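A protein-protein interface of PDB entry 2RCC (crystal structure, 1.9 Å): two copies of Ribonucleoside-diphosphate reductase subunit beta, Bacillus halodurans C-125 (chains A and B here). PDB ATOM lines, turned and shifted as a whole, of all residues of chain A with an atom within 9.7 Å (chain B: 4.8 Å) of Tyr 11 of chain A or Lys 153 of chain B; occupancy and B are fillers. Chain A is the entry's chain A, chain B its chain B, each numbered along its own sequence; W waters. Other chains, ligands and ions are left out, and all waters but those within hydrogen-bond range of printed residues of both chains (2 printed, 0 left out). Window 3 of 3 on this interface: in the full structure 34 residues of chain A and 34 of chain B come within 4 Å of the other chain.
OE2 of Glu 157 of chain B is in hydrogen-bond range of OH of Tyr 11 of chain A, 2.7 Å away. The side-chain amino group of Lys 147 of chain B is in hydrogen-bond range of the side-chain amide oxygen of Asn 17 of chain A. The backbone carbonyl oxygen (O) of Ala 15 of chain A sits at hydrogen-bond distance from the side-chain amino group (NZ) of Lys 147 of chain B (3.1 Å).
The backbone carbonyl oxygen (O) of Ser 28 of chain A is in hydrogen-bond range of the backbone NH (N) of Asp 12 of chain A (3.2 Å). The side-chain amide oxygen (OD1) of Asn 17 of chain A is in hydrogen-bond range of the side-chain hydroxyl (OG) of Ser 28 of chain A, at 2.6 Å. The side-chain hydroxyl of Thr 14 of chain A lies within hydrogen-bond range of the side-chain carboxylate of Asp 12 of chain A (2.6 Å). The side-chain amino group (NZ) of Lys 153 of chain B is in hydrogen-bond range of the backbone carbonyl oxygen (O) of Lys 147 of chain B. The backbone carbonyl oxygen (O) of Ile 10 of chain A sits at hydrogen-bond distance from the side-chain amide nitrogen (ND2) of Asn 29 of chain A (2.9 Å). The backbone NH (N) of Val 30 of chain A is in hydrogen-bond range of the side-chain hydroxyl (OG) of Ser 28 of chain A (3.1 Å).
Glu 164 of chain B touches Ile 10 of chain A. Tyr 11 of chain A touches Phe 87 of chain B. Lys 153 of chain B touches Tyr 11 of chain A. Tyr 11 of chain A touches Ile 160 of chain B (CG to CG1, 3.7 Å). Asp 12 of chain A touches Trp 146 of chain B (O to CH2, 3.5 Å). CG2 of Thr 13 of chain A touches CZ3 of Trp 146 of chain B, at 3.5 Å. Ser 16 of chain A touches Lys 147 of chain B (CA to NZ, 3.6 Å). OD1 of Asn 17 of chain A touches CZ2 of Trp 146 of chain B, at 3.8 Å. CB of Ser 28 of chain A touches CZ2 of Trp 146 of chain B, at 3.3 Å. Val 30 of chain A touches Trp 146 of chain B.
Lys 7 of chain A touches none of the printed residues of chain B. Lys 9 of chain A touches none of the printed residues of chain B. Printed residues of chain B within 4 Å of Ser 16 of chain A: Lys 147 (3.6 Å). Of the printed residues of chain B, Val 30 of chain A touches Phe 87 and Trp 146. Of the printed residues of chain A, Lys 147 of chain B touches Ala 15 (3.1 Å), Ser 16 (3.6 Å) and Asn 17 (3.4 Å). No residue of chain A comes within 4 Å of Leu 152 of chain B. Lys 153 of chain B touches just one residue of chain A: Tyr 11 (3.8 Å). No residue of chain A comes within 4 Å of Asn 156 of chain B. Of the printed residues of chain A, Glu 157 of chain B touches Tyr 11 (2.7 Å). The nearest residue of chain B that does not touch Tyr 11 of chain A is Glu 164 of chain B (4.6 Å). The nearest residue of chain A that does not touch Lys 153 of chain B is Thr 13 of chain A (4.5 Å). The nearest printed residue of chain B that does not touch Asn 17 of chain A is Phe 87 of chain B (8.0 Å).
Of the 14 printed residues of chain B, 7 touch a printed residue of chain A. Hydrophobic or aromatic side chains of chain B within 4 Å of the printed part of chain A: Phe 87, Trp 146 and Ile 160. Of the 17 printed residues of chain A, 9 touch a printed residue of chain B. Among the printed residues, 15 pairs touch across the chains.
No position is printed for both chains.
Water W2 lies within hydrogen-bond range of OH of Tyr 11 of chain A (2.8 Å), O of Trp 146 of chain B (2.9 Å) and ND2 of Asn 156 of chain B (2.9 Å). Water W1 bridges the backbone NH of Asn 17 of chain A and the side-chain amino group of Lys 147 of chain B.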
ATOM      1  N   LYS A   7      -8.081   4.921  27.717  1.00  0.00           N
ATOM      2  CA  LYS A   7      -8.494   5.801  26.647  1.00  0.00           C
ATOM      3  C   LYS A   7      -9.096   5.028  25.491  1.00  0.00           C
ATOM      4  O   LYS A   7      -8.712   3.890  25.247  1.00  0.00           O
ATOM      5  CB  LYS A   7      -7.321   6.654  26.109  1.00  0.00           C
ATOM      6  CG  LYS A   7      -6.979   7.906  26.920  1.00  0.00           C
ATOM      7  CD  LYS A   7      -5.790   8.622  26.324  1.00  0.00           C
ATOM      8  CE  LYS A   7      -5.321   9.837  27.160  1.00  0.00           C
ATOM      9  N   ARG A   8     -10.023   5.668  24.777  1.00  0.00           N
ATOM     10  CA  ARG A   8     -10.611   5.091  23.575  1.00  0.00           C
ATOM     11  C   ARG A   8      -9.546   4.833  22.518  1.00  0.00           C
ATOM     12  O   ARG A   8      -8.726   5.708  22.204  1.00  0.00           O
ATOM     13  CB  ARG A   8     -11.641   6.028  22.985  1.00  0.00           C
ATOM     14  CG  ARG A   8     -12.250   5.600  21.633  1.00  0.00           C
ATOM     15  CD  ARG A   8     -13.273   6.572  21.117  1.00  0.00           C
ATOM     16  NE  ARG A   8     -12.777   7.936  20.906  1.00  0.00           N
ATOM     17  CZ  ARG A   8     -12.900   8.959  21.754  1.00  0.00           C
ATOM     18  NH1 ARG A   8     -13.565   8.879  22.896  1.00  0.00           N
ATOM     19  NH2 ARG A   8     -12.395  10.126  21.426  1.00  0.00           N
ATOM     20  N   LYS A   9      -9.580   3.641  21.951  1.00  0.00           N
ATOM     21  CA  LYS A   9      -8.682   3.276  20.865  1.00  0.00           C
ATOM     22  C   LYS A   9      -9.223   3.892  19.585  1.00  0.00           C
ATOM     23  O   LYS A   9     -10.407   3.734  19.269  1.00  0.00           O
ATOM     24  CB  LYS A   9      -8.571   1.754  20.683  1.00  0.00           C
ATOM     25  CG  LYS A   9      -7.826   1.078  21.817  1.00  0.00           C
ATOM     26  CD  LYS A   9      -7.579  -0.415  21.481  1.00  0.00           C
ATOM     27  N   ILE A  10      -8.340   4.500  18.800  1.00  0.00           N
ATOM     28  CA  ILE A  10      -8.748   5.128  17.550  1.00  0.00           C
ATOM     29  C   ILE A  10      -9.148   4.081  16.479  1.00  0.00           C
ATOM     30  O   ILE A  10      -9.827   4.420  15.503  1.00  0.00           O
ATOM     31  CB  ILE A  10      -7.639   6.117  17.056  1.00  0.00           C
ATOM     32  CG1 ILE A  10      -8.214   7.220  16.156  1.00  0.00           C
ATOM     33  CG2 ILE A  10      -6.502   5.358  16.397  1.00  0.00           C
ATOM     34  CD1 ILE A  10      -7.244   8.371  15.916  1.00  0.00           C
ATOM     35  N   TYR A  11      -8.763   2.820  16.691  1.00  0.00           N
ATOM     36  CA  TYR A  11      -8.959   1.696  15.775  1.00  0.00           C
ATOM     37  C   TYR A  11      -8.813   0.369  16.542  1.00  0.00           C
ATOM     38  O   TYR A  11      -7.810   0.156  17.226  1.00  0.00           O
ATOM     39  CB  TYR A  11      -7.849   1.762  14.738  1.00  0.00           C
ATOM     40  CG  TYR A  11      -7.730   0.645  13.723  1.00  0.00           C
ATOM     41  CD1 TYR A  11      -8.616   0.552  12.674  1.00  0.00           C
ATOM     42  CD2 TYR A  11      -6.664  -0.248  13.747  1.00  0.00           C
ATOM     43  CE1 TYR A  11      -8.483  -0.422  11.702  1.00  0.00           C
ATOM     44  CE2 TYR A  11      -6.521  -1.217  12.769  1.00  0.00           C
ATOM     45  CZ  TYR A  11      -7.442  -1.301  11.744  1.00  0.00           C
ATOM     46  OH  TYR A  11      -7.326  -2.254  10.737  1.00  0.00           O
ATOM     47  N   ASP A  12      -9.824  -0.478  16.478  1.00  0.00           N
ATOM     48  CA  ASP A  12      -9.794  -1.794  17.135  1.00  0.00           C
ATOM     49  C   ASP A  12     -10.537  -2.823  16.257  1.00  0.00           C
ATOM     50  O   ASP A  12     -11.760  -2.847  16.195  1.00  0.00           O
ATOM     51  CB  ASP A  12     -10.389  -1.662  18.538  1.00  0.00           C
ATOM     52  CG  ASP A  12     -10.306  -2.933  19.351  1.00  0.00           C
ATOM     53  OD1 ASP A  12      -9.831  -3.961  18.871  1.00  0.00           O
ATOM     54  OD2 ASP A  12     -10.720  -2.899  20.504  1.00  0.00           O
ATOM     55  N   THR A  13      -9.776  -3.680  15.576  1.00  0.00           N
ATOM     56  CA  THR A  13     -10.360  -4.709  14.704  1.00  0.00           C
ATOM     57  C   THR A  13     -11.033  -5.851  15.470  1.00  0.00           C
ATOM     58  O   THR A  13     -11.908  -6.516  14.926  1.00  0.00           O
ATOM     59  CB  THR A  13      -9.302  -5.337  13.742  1.00  0.00           C
ATOM     60  OG1 THR A  13      -8.214  -5.840  14.522  1.00  0.00           O
ATOM     61  CG2 THR A  13      -8.799  -4.302  12.735  1.00  0.00           C
ATOM     62  N   THR A  14     -10.648  -6.035  16.733  1.00  0.00           N
ATOM     63  CA  THR A  14     -11.207  -7.070  17.576  1.00  0.00           C
ATOM     64  C   THR A  14     -12.608  -6.704  18.127  1.00  0.00           C
ATOM     65  O   THR A  14     -13.259  -7.566  18.699  1.00  0.00           O
ATOM     66  CB  THR A  14     -10.306  -7.380  18.806  1.00  0.00           C
ATOM     67  OG1 THR A  14     -10.451  -6.351  19.784  1.00  0.00           O
ATOM     68  CG2 THR A  14      -8.819  -7.532  18.434  1.00  0.00           C
ATOM     69  N   ALA A  15     -13.085  -5.469  17.944  1.00  0.00           N
ATOM     70  CA  ALA A  15     -14.359  -5.035  18.503  1.00  0.00           C
ATOM     71  C   ALA A  15     -15.461  -4.815  17.456  1.00  0.00           C
ATOM     72  O   ALA A  15     -15.199  -4.675  16.255  1.00  0.00           O
ATOM     73  CB  ALA A  15     -14.135  -3.750  19.317  1.00  0.00           C
ATOM     74  N   SER A  16     -16.702  -4.812  17.942  1.00  0.00           N
ATOM     75  CA  SER A  16     -17.887  -4.506  17.156  1.00  0.00           C
ATOM     76  C   SER A  16     -18.034  -2.967  16.979  1.00  0.00           C
ATOM     77  O   SER A  16     -17.438  -2.188  17.727  1.00  0.00           O
ATOM     78  CB  SER A  16     -19.108  -5.068  17.860  1.00  0.00           C
ATOM     79  OG  SER A  16     -19.228  -4.584  19.208  1.00  0.00           O
ATOM     80  N   ASN A  17     -18.817  -2.545  15.982  1.00  0.00           N
ATOM     81  CA  ASN A  17     -19.064  -1.123  15.744  1.00  0.00           C
ATOM     82  C   ASN A  17     -19.937  -0.531  16.832  1.00  0.00           C
ATOM     83  O   ASN A  17     -19.683   0.607  17.250  1.00  0.00           O
ATOM     84  CB  ASN A  17     -19.676  -0.893  14.334  1.00  0.00           C
ATOM     85  CG  ASN A  17     -18.750  -1.360  13.189  1.00  0.00           C
ATOM     86  OD1 ASN A  17     -17.540  -1.544  13.379  1.00  0.00           O
ATOM     87  ND2 ASN A  17     -19.329  -1.521  11.984  1.00  0.00           N
ATOM     88  N   LYS A  26     -15.573  -2.020  24.593  1.00  0.00           N
ATOM     89  CA  LYS A  26     -14.939  -2.341  23.324  1.00  0.00           C
ATOM     90  C   LYS A  26     -15.775  -1.688  22.240  1.00  0.00           C
ATOM     91  O   LYS A  26     -17.004  -1.740  22.308  1.00  0.00           O
ATOM     92  CB  LYS A  26     -14.910  -3.842  23.106  1.00  0.00           C
ATOM     93  CG  LYS A  26     -14.100  -4.619  24.120  1.00  0.00           C
ATOM     94  CD  LYS A  26     -12.604  -4.407  23.927  1.00  0.00           C
ATOM     95  CE  LYS A  26     -11.804  -5.439  24.750  1.00  0.00           C
ATOM     96  N   SER A  27     -15.085  -1.086  21.279  1.00  0.00           N
ATOM     97  CA  SER A  27     -15.661  -0.390  20.147  1.00  0.00           C
ATOM     98  C   SER A  27     -14.633  -0.399  19.022  1.00  0.00           C
ATOM     99  O   SER A  27     -13.450  -0.092  19.240  1.00  0.00           O
ATOM    100  CB  SER A  27     -15.926   1.073  20.536  1.00  0.00           C
ATOM    101  OG  SER A  27     -16.502   1.793  19.436  1.00  0.00           O
ATOM    102  N   SER A  28     -15.071  -0.630  17.793  1.00  0.00           N
ATOM    103  CA  SER A  28     -14.152  -0.569  16.677  1.00  0.00           C
ATOM    104  C   SER A  28     -13.636   0.809  16.347  1.00  0.00           C
ATOM    105  O   SER A  28     -12.554   0.947  15.795  1.00  0.00           O
ATOM    106  CB  SER A  28     -14.802  -1.074  15.411  1.00  0.00           C
ATOM    107  OG  SER A  28     -15.909  -0.326  15.007  1.00  0.00           O
ATOM    108  N   ASN A  29     -14.461   1.795  16.678  1.00  0.00           N
ATOM    109  CA  ASN A  29     -14.314   3.214  16.406  1.00  0.00           C
ATOM    110  C   ASN A  29     -14.783   3.604  14.973  1.00  0.00           C
ATOM    111  O   ASN A  29     -14.633   4.734  14.568  1.00  0.00           O
ATOM    112  CB  ASN A  29     -12.929   3.758  16.734  1.00  0.00           C
ATOM    113  CG  ASN A  29     -12.979   5.227  17.102  1.00  0.00           C
ATOM    114  OD1 ASN A  29     -13.918   5.653  17.763  1.00  0.00           O
ATOM    115  ND2 ASN A  29     -11.999   6.010  16.647  1.00  0.00           N
ATOM    116  N   VAL A  30     -15.354   2.651  14.229  1.00  0.00           N
ATOM    117  CA  VAL A  30     -15.980   2.914  12.946  1.00  0.00           C
ATOM    118  C   VAL A  30     -17.451   3.063  13.288  1.00  0.00           C
ATOM    119  O   VAL A  30     -18.050   2.154  13.885  1.00  0.00           O
ATOM    120  CB  VAL A  30     -15.795   1.755  11.962  1.00  0.00           C
ATOM    121  CG1 VAL A  30     -16.523   2.053  10.651  1.00  0.00           C
ATOM    122  CG2 VAL A  30     -14.313   1.502  11.704  1.00  0.00           C
ATOM    123  N   SER A 106     -18.270   5.171  19.962  1.00  0.00           N
ATOM    124  CA  SER A 106     -17.969   6.082  18.863  1.00  0.00           C
ATOM    125  C   SER A 106     -19.075   7.090  18.628  1.00  0.00           C
ATOM    126  O   SER A 106     -18.779   8.223  18.198  1.00  0.00           O
ATOM    127  CB  SER A 106     -17.659   5.331  17.569  1.00  0.00           C
ATOM    128  OG  SER A 106     -18.716   4.483  17.202  1.00  0.00           O
ATOM    129  N   PHE B  87     -14.855   4.543   6.998  1.00  0.00           N
ATOM    130  CA  PHE B  87     -13.714   4.211   7.878  1.00  0.00           C
ATOM    131  C   PHE B  87     -12.858   5.454   8.077  1.00  0.00           C
ATOM    132  O   PHE B  87     -12.542   5.805   9.205  1.00  0.00           O
ATOM    133  CB  PHE B  87     -12.821   3.075   7.291  1.00  0.00           C
ATOM    134  CG  PHE B  87     -11.605   2.799   8.130  1.00  0.00           C
ATOM    135  CD1 PHE B  87     -11.703   1.970   9.194  1.00  0.00           C
ATOM    136  CD2 PHE B  87     -10.392   3.452   7.907  1.00  0.00           C
ATOM    137  CE1 PHE B  87     -10.611   1.774  10.059  1.00  0.00           C
ATOM    138  CE2 PHE B  87      -9.322   3.259   8.751  1.00  0.00           C
ATOM    139  CZ  PHE B  87      -9.439   2.421   9.823  1.00  0.00           C
ATOM    140  N   TRP B 146     -13.780  -3.194   6.395  1.00  0.00           N
ATOM    141  CA  TRP B 146     -12.493  -2.807   6.954  1.00  0.00           C
ATOM    142  C   TRP B 146     -11.849  -3.895   7.871  1.00  0.00           C
ATOM    143  O   TRP B 146     -10.626  -3.934   8.005  1.00  0.00           O
ATOM    144  CB  TRP B 146     -12.628  -1.442   7.664  1.00  0.00           C
ATOM    145  CG  TRP B 146     -13.434  -1.523   8.882  1.00  0.00           C
ATOM    146  CD1 TRP B 146     -14.784  -1.449   8.993  1.00  0.00           C
ATOM    147  CD2 TRP B 146     -12.939  -1.771  10.169  1.00  0.00           C
ATOM    148  NE1 TRP B 146     -15.153  -1.605  10.296  1.00  0.00           N
ATOM    149  CE2 TRP B 146     -14.032  -1.816  11.033  1.00  0.00           C
ATOM    150  CE3 TRP B 146     -11.661  -1.969  10.686  1.00  0.00           C
ATOM    151  CZ2 TRP B 146     -13.894  -2.031  12.358  1.00  0.00           C
ATOM    152  CZ3 TRP B 146     -11.522  -2.170  11.999  1.00  0.00           C
ATOM    153  CH2 TRP B 146     -12.631  -2.212  12.839  1.00  0.00           C
ATOM    154  N   LYS B 147     -12.657  -4.747   8.498  1.00  0.00           N
ATOM    155  CA  LYS B 147     -12.150  -5.818   9.363  1.00  0.00           C
ATOM    156  C   LYS B 147     -11.817  -7.066   8.552  1.00  0.00           C
ATOM    157  O   LYS B 147     -10.974  -7.826   8.986  1.00  0.00           O
ATOM    158  CB  LYS B 147     -13.166  -6.269  10.417  1.00  0.00           C
ATOM    159  CG  LYS B 147     -13.781  -5.203  11.268  1.00  0.00           C
ATOM    160  CD  LYS B 147     -14.861  -5.776  12.240  1.00  0.00           C
ATOM    161  CE  LYS B 147     -15.624  -4.628  12.952  1.00  0.00           C
ATOM    162  NZ  LYS B 147     -16.889  -4.890  13.701  1.00  0.00           N
ATOM    163  N   ASP B 149     -11.413  -7.400   4.699  1.00  0.00           N
ATOM    164  CA  ASP B 149     -10.693  -7.316   3.426  1.00  0.00           C
ATOM    165  C   ASP B 149      -9.231  -6.977   3.708  1.00  0.00           C
ATOM    166  O   ASP B 149      -8.942  -5.905   4.249  1.00  0.00           O
ATOM    167  CB  ASP B 149     -11.382  -6.274   2.548  1.00  0.00           C
ATOM    168  CG  ASP B 149     -10.770  -6.152   1.173  1.00  0.00           C
ATOM    169  OD1 ASP B 149      -9.620  -5.708   1.074  1.00  0.00           O
ATOM    170  OD2 ASP B 149     -11.478  -6.420   0.185  1.00  0.00           O
ATOM    171  N   ASP B 150      -8.313  -7.874   3.335  1.00  0.00           N
ATOM    172  CA  ASP B 150      -6.886  -7.666   3.580  1.00  0.00           C
ATOM    173  C   ASP B 150      -6.301  -6.458   2.829  1.00  0.00           C
ATOM    174  O   ASP B 150      -5.346  -5.870   3.314  1.00  0.00           O
ATOM    175  CB  ASP B 150      -6.064  -8.920   3.226  1.00  0.00           C
ATOM    176  CG  ASP B 150      -6.299 -10.075   4.190  1.00  0.00           C
ATOM    177  OD1 ASP B 150      -6.237  -9.875   5.432  1.00  0.00           O
ATOM    178  OD2 ASP B 150      -6.506 -11.198   3.685  1.00  0.00           O
ATOM    179  N   VAL B 151      -6.865  -6.115   1.665  1.00  0.00           N
ATOM    180  CA  VAL B 151      -6.400  -4.968   0.910  1.00  0.00           C
ATOM    181  C   VAL B 151      -6.819  -3.686   1.651  1.00  0.00           C
ATOM    182  O   VAL B 151      -5.989  -2.793   1.864  1.00  0.00           O
ATOM    183  CB  VAL B 151      -6.917  -4.979  -0.566  1.00  0.00           C
ATOM    184  CG1 VAL B 151      -6.488  -3.723  -1.304  1.00  0.00           C
ATOM    185  CG2 VAL B 151      -6.436  -6.269  -1.314  1.00  0.00           C
ATOM    186  N   LEU B 152      -8.087  -3.603   2.066  1.00  0.00           N
ATOM    187  CA  LEU B 152      -8.559  -2.423   2.793  1.00  0.00           C
ATOM    188  C   LEU B 152      -7.826  -2.299   4.134  1.00  0.00           C
ATOM    189  O   LEU B 152      -7.419  -1.203   4.537  1.00  0.00           O
ATOM    190  CB  LEU B 152     -10.090  -2.448   2.967  1.00  0.00           C
ATOM    191  CG  LEU B 152     -10.806  -1.238   3.574  1.00  0.00           C
ATOM    192  CD1 LEU B 152     -10.452   0.086   2.862  1.00  0.00           C
ATOM    193  CD2 LEU B 152     -12.318  -1.454   3.628  1.00  0.00           C
ATOM    194  N   LYS B 153      -7.596  -3.423   4.789  1.00  0.00           N
ATOM    195  CA  LYS B 153      -6.893  -3.404   6.052  1.00  0.00           C
ATOM    196  C   LYS B 153      -5.458  -2.904   5.898  1.00  0.00           C
ATOM    197  O   LYS B 153      -4.988  -2.115   6.708  1.00  0.00           O
ATOM    198  CB  LYS B 153      -6.961  -4.772   6.702  1.00  0.00           C
ATOM    199  CG  LYS B 153      -6.447  -4.816   8.104  1.00  0.00           C
ATOM    200  CD  LYS B 153      -6.527  -6.208   8.722  1.00  0.00           C
ATOM    201  CE  LYS B 153      -7.913  -6.645   8.974  1.00  0.00           C
ATOM    202  NZ  LYS B 153      -7.853  -7.857   9.818  1.00  0.00           N
ATOM    203  N   GLU B 154      -4.757  -3.357   4.854  1.00  0.00           N
ATOM    204  CA  GLU B 154      -3.385  -2.909   4.625  1.00  0.00           C
ATOM    205  C   GLU B 154      -3.302  -1.391   4.524  1.00  0.00           C
ATOM    206  O   GLU B 154      -2.493  -0.737   5.207  1.00  0.00           O
ATOM    207  CB  GLU B 154      -2.807  -3.568   3.355  1.00  0.00           C
ATOM    208  CG  GLU B 154      -1.489  -2.980   2.918  1.00  0.00           C
ATOM    209  CD  GLU B 154      -0.819  -3.765   1.797  1.00  0.00           C
ATOM    210  OE1 GLU B 154      -1.475  -4.090   0.789  1.00  0.00           O
ATOM    211  OE2 GLU B 154       0.388  -4.006   1.929  1.00  0.00           O
ATOM    212  N   ARG B 155      -4.119  -0.836   3.649  1.00  0.00           N
ATOM    213  CA  ARG B 155      -4.111   0.602   3.466  1.00  0.00           C
ATOM    214  C   ARG B 155      -4.552   1.371   4.720  1.00  0.00           C
ATOM    215  O   ARG B 155      -3.948   2.378   5.064  1.00  0.00           O
ATOM    216  CB  ARG B 155      -4.899   0.995   2.211  1.00  0.00           C
ATOM    217  CG  ARG B 155      -6.386   0.720   2.191  1.00  0.00           C
ATOM    218  CD  ARG B 155      -7.035   1.376   0.963  1.00  0.00           C
ATOM    219  NE  ARG B 155      -6.991   2.830   1.104  1.00  0.00           N
ATOM    220  CZ  ARG B 155      -7.163   3.735   0.149  1.00  0.00           C
ATOM    221  NH1 ARG B 155      -7.451   3.376  -1.070  1.00  0.00           N
ATOM    222  NH2 ARG B 155      -7.049   5.017   0.451  1.00  0.00           N
ATOM    223  N   ASN B 156      -5.583   0.887   5.405  1.00  0.00           N
ATOM    224  CA  ASN B 156      -6.088   1.533   6.639  1.00  0.00           C
ATOM    225  C   ASN B 156      -5.031   1.584   7.743  1.00  0.00           C
ATOM    226  O   ASN B 156      -4.891   2.594   8.401  1.00  0.00           O
ATOM    227  CB  ASN B 156      -7.347   0.825   7.174  1.00  0.00           C
ATOM    228  CG  ASN B 156      -8.593   1.086   6.313  1.00  0.00           C
ATOM    229  OD1 ASN B 156      -8.596   1.960   5.474  1.00  0.00           O
ATOM    230  ND2 ASN B 156      -9.647   0.375   6.581  1.00  0.00           N
ATOM    231  N   GLU B 157      -4.255   0.520   7.879  1.00  0.00           N
ATOM    232  CA  GLU B 157      -3.239   0.433   8.943  1.00  0.00           C
ATOM    233  C   GLU B 157      -2.049   1.362   8.700  1.00  0.00           C
ATOM    234  O   GLU B 157      -1.385   1.760   9.666  1.00  0.00           O
ATOM    235  CB  GLU B 157      -2.881  -1.040   9.228  1.00  0.00           C
ATOM    236  CG  GLU B 157      -4.127  -1.712   9.883  1.00  0.00           C
ATOM    237  CD  GLU B 157      -4.085  -3.202  10.118  1.00  0.00           C
ATOM    238  OE1 GLU B 157      -3.125  -3.871   9.625  1.00  0.00           O
ATOM    239  OE2 GLU B 157      -5.085  -3.701  10.772  1.00  0.00           O
ATOM    240  N   ILE B 160      -3.569   4.501  10.249  1.00  0.00           N
ATOM    241  CA  ILE B 160      -3.658   4.334  11.713  1.00  0.00           C
ATOM    242  C   ILE B 160      -2.295   4.434  12.411  1.00  0.00           C
ATOM    243  O   ILE B 160      -2.176   5.107  13.436  1.00  0.00           O
ATOM    244  CB  ILE B 160      -4.380   3.004  12.107  1.00  0.00           C
ATOM    245  CG1 ILE B 160      -5.850   3.038  11.646  1.00  0.00           C
ATOM    246  CG2 ILE B 160      -4.289   2.736  13.617  1.00  0.00           C
ATOM    247  CD1 ILE B 160      -6.671   4.352  12.020  1.00  0.00           C
ATOM    248  N   GLU B 164      -1.662   6.988  15.330  1.00  0.00           N
ATOM    249  CA  GLU B 164      -1.335   6.410  16.646  1.00  0.00           C
ATOM    250  C   GLU B 164      -0.024   6.905  17.233  1.00  0.00           C
ATOM    251  O   GLU B 164       0.076   7.088  18.446  1.00  0.00           O
ATOM    252  CB  GLU B 164      -1.350   4.875  16.597  1.00  0.00           C
ATOM    253  CG  GLU B 164      -2.744   4.305  16.581  1.00  0.00           C
ATOM    254  CD  GLU B 164      -2.783   2.764  16.690  1.00  0.00           C
ATOM    255  OE1 GLU B 164      -1.858   2.092  16.170  1.00  0.00           O
ATOM    256  OE2 GLU B 164      -3.756   2.251  17.286  1.00  0.00           O
HETATM  257  O   HOH W   1     -19.862  -4.664  14.263  1.00  0.00           O
HETATM  258  O   HOH W   2      -8.855  -1.691   8.491  1.00  0.00           O
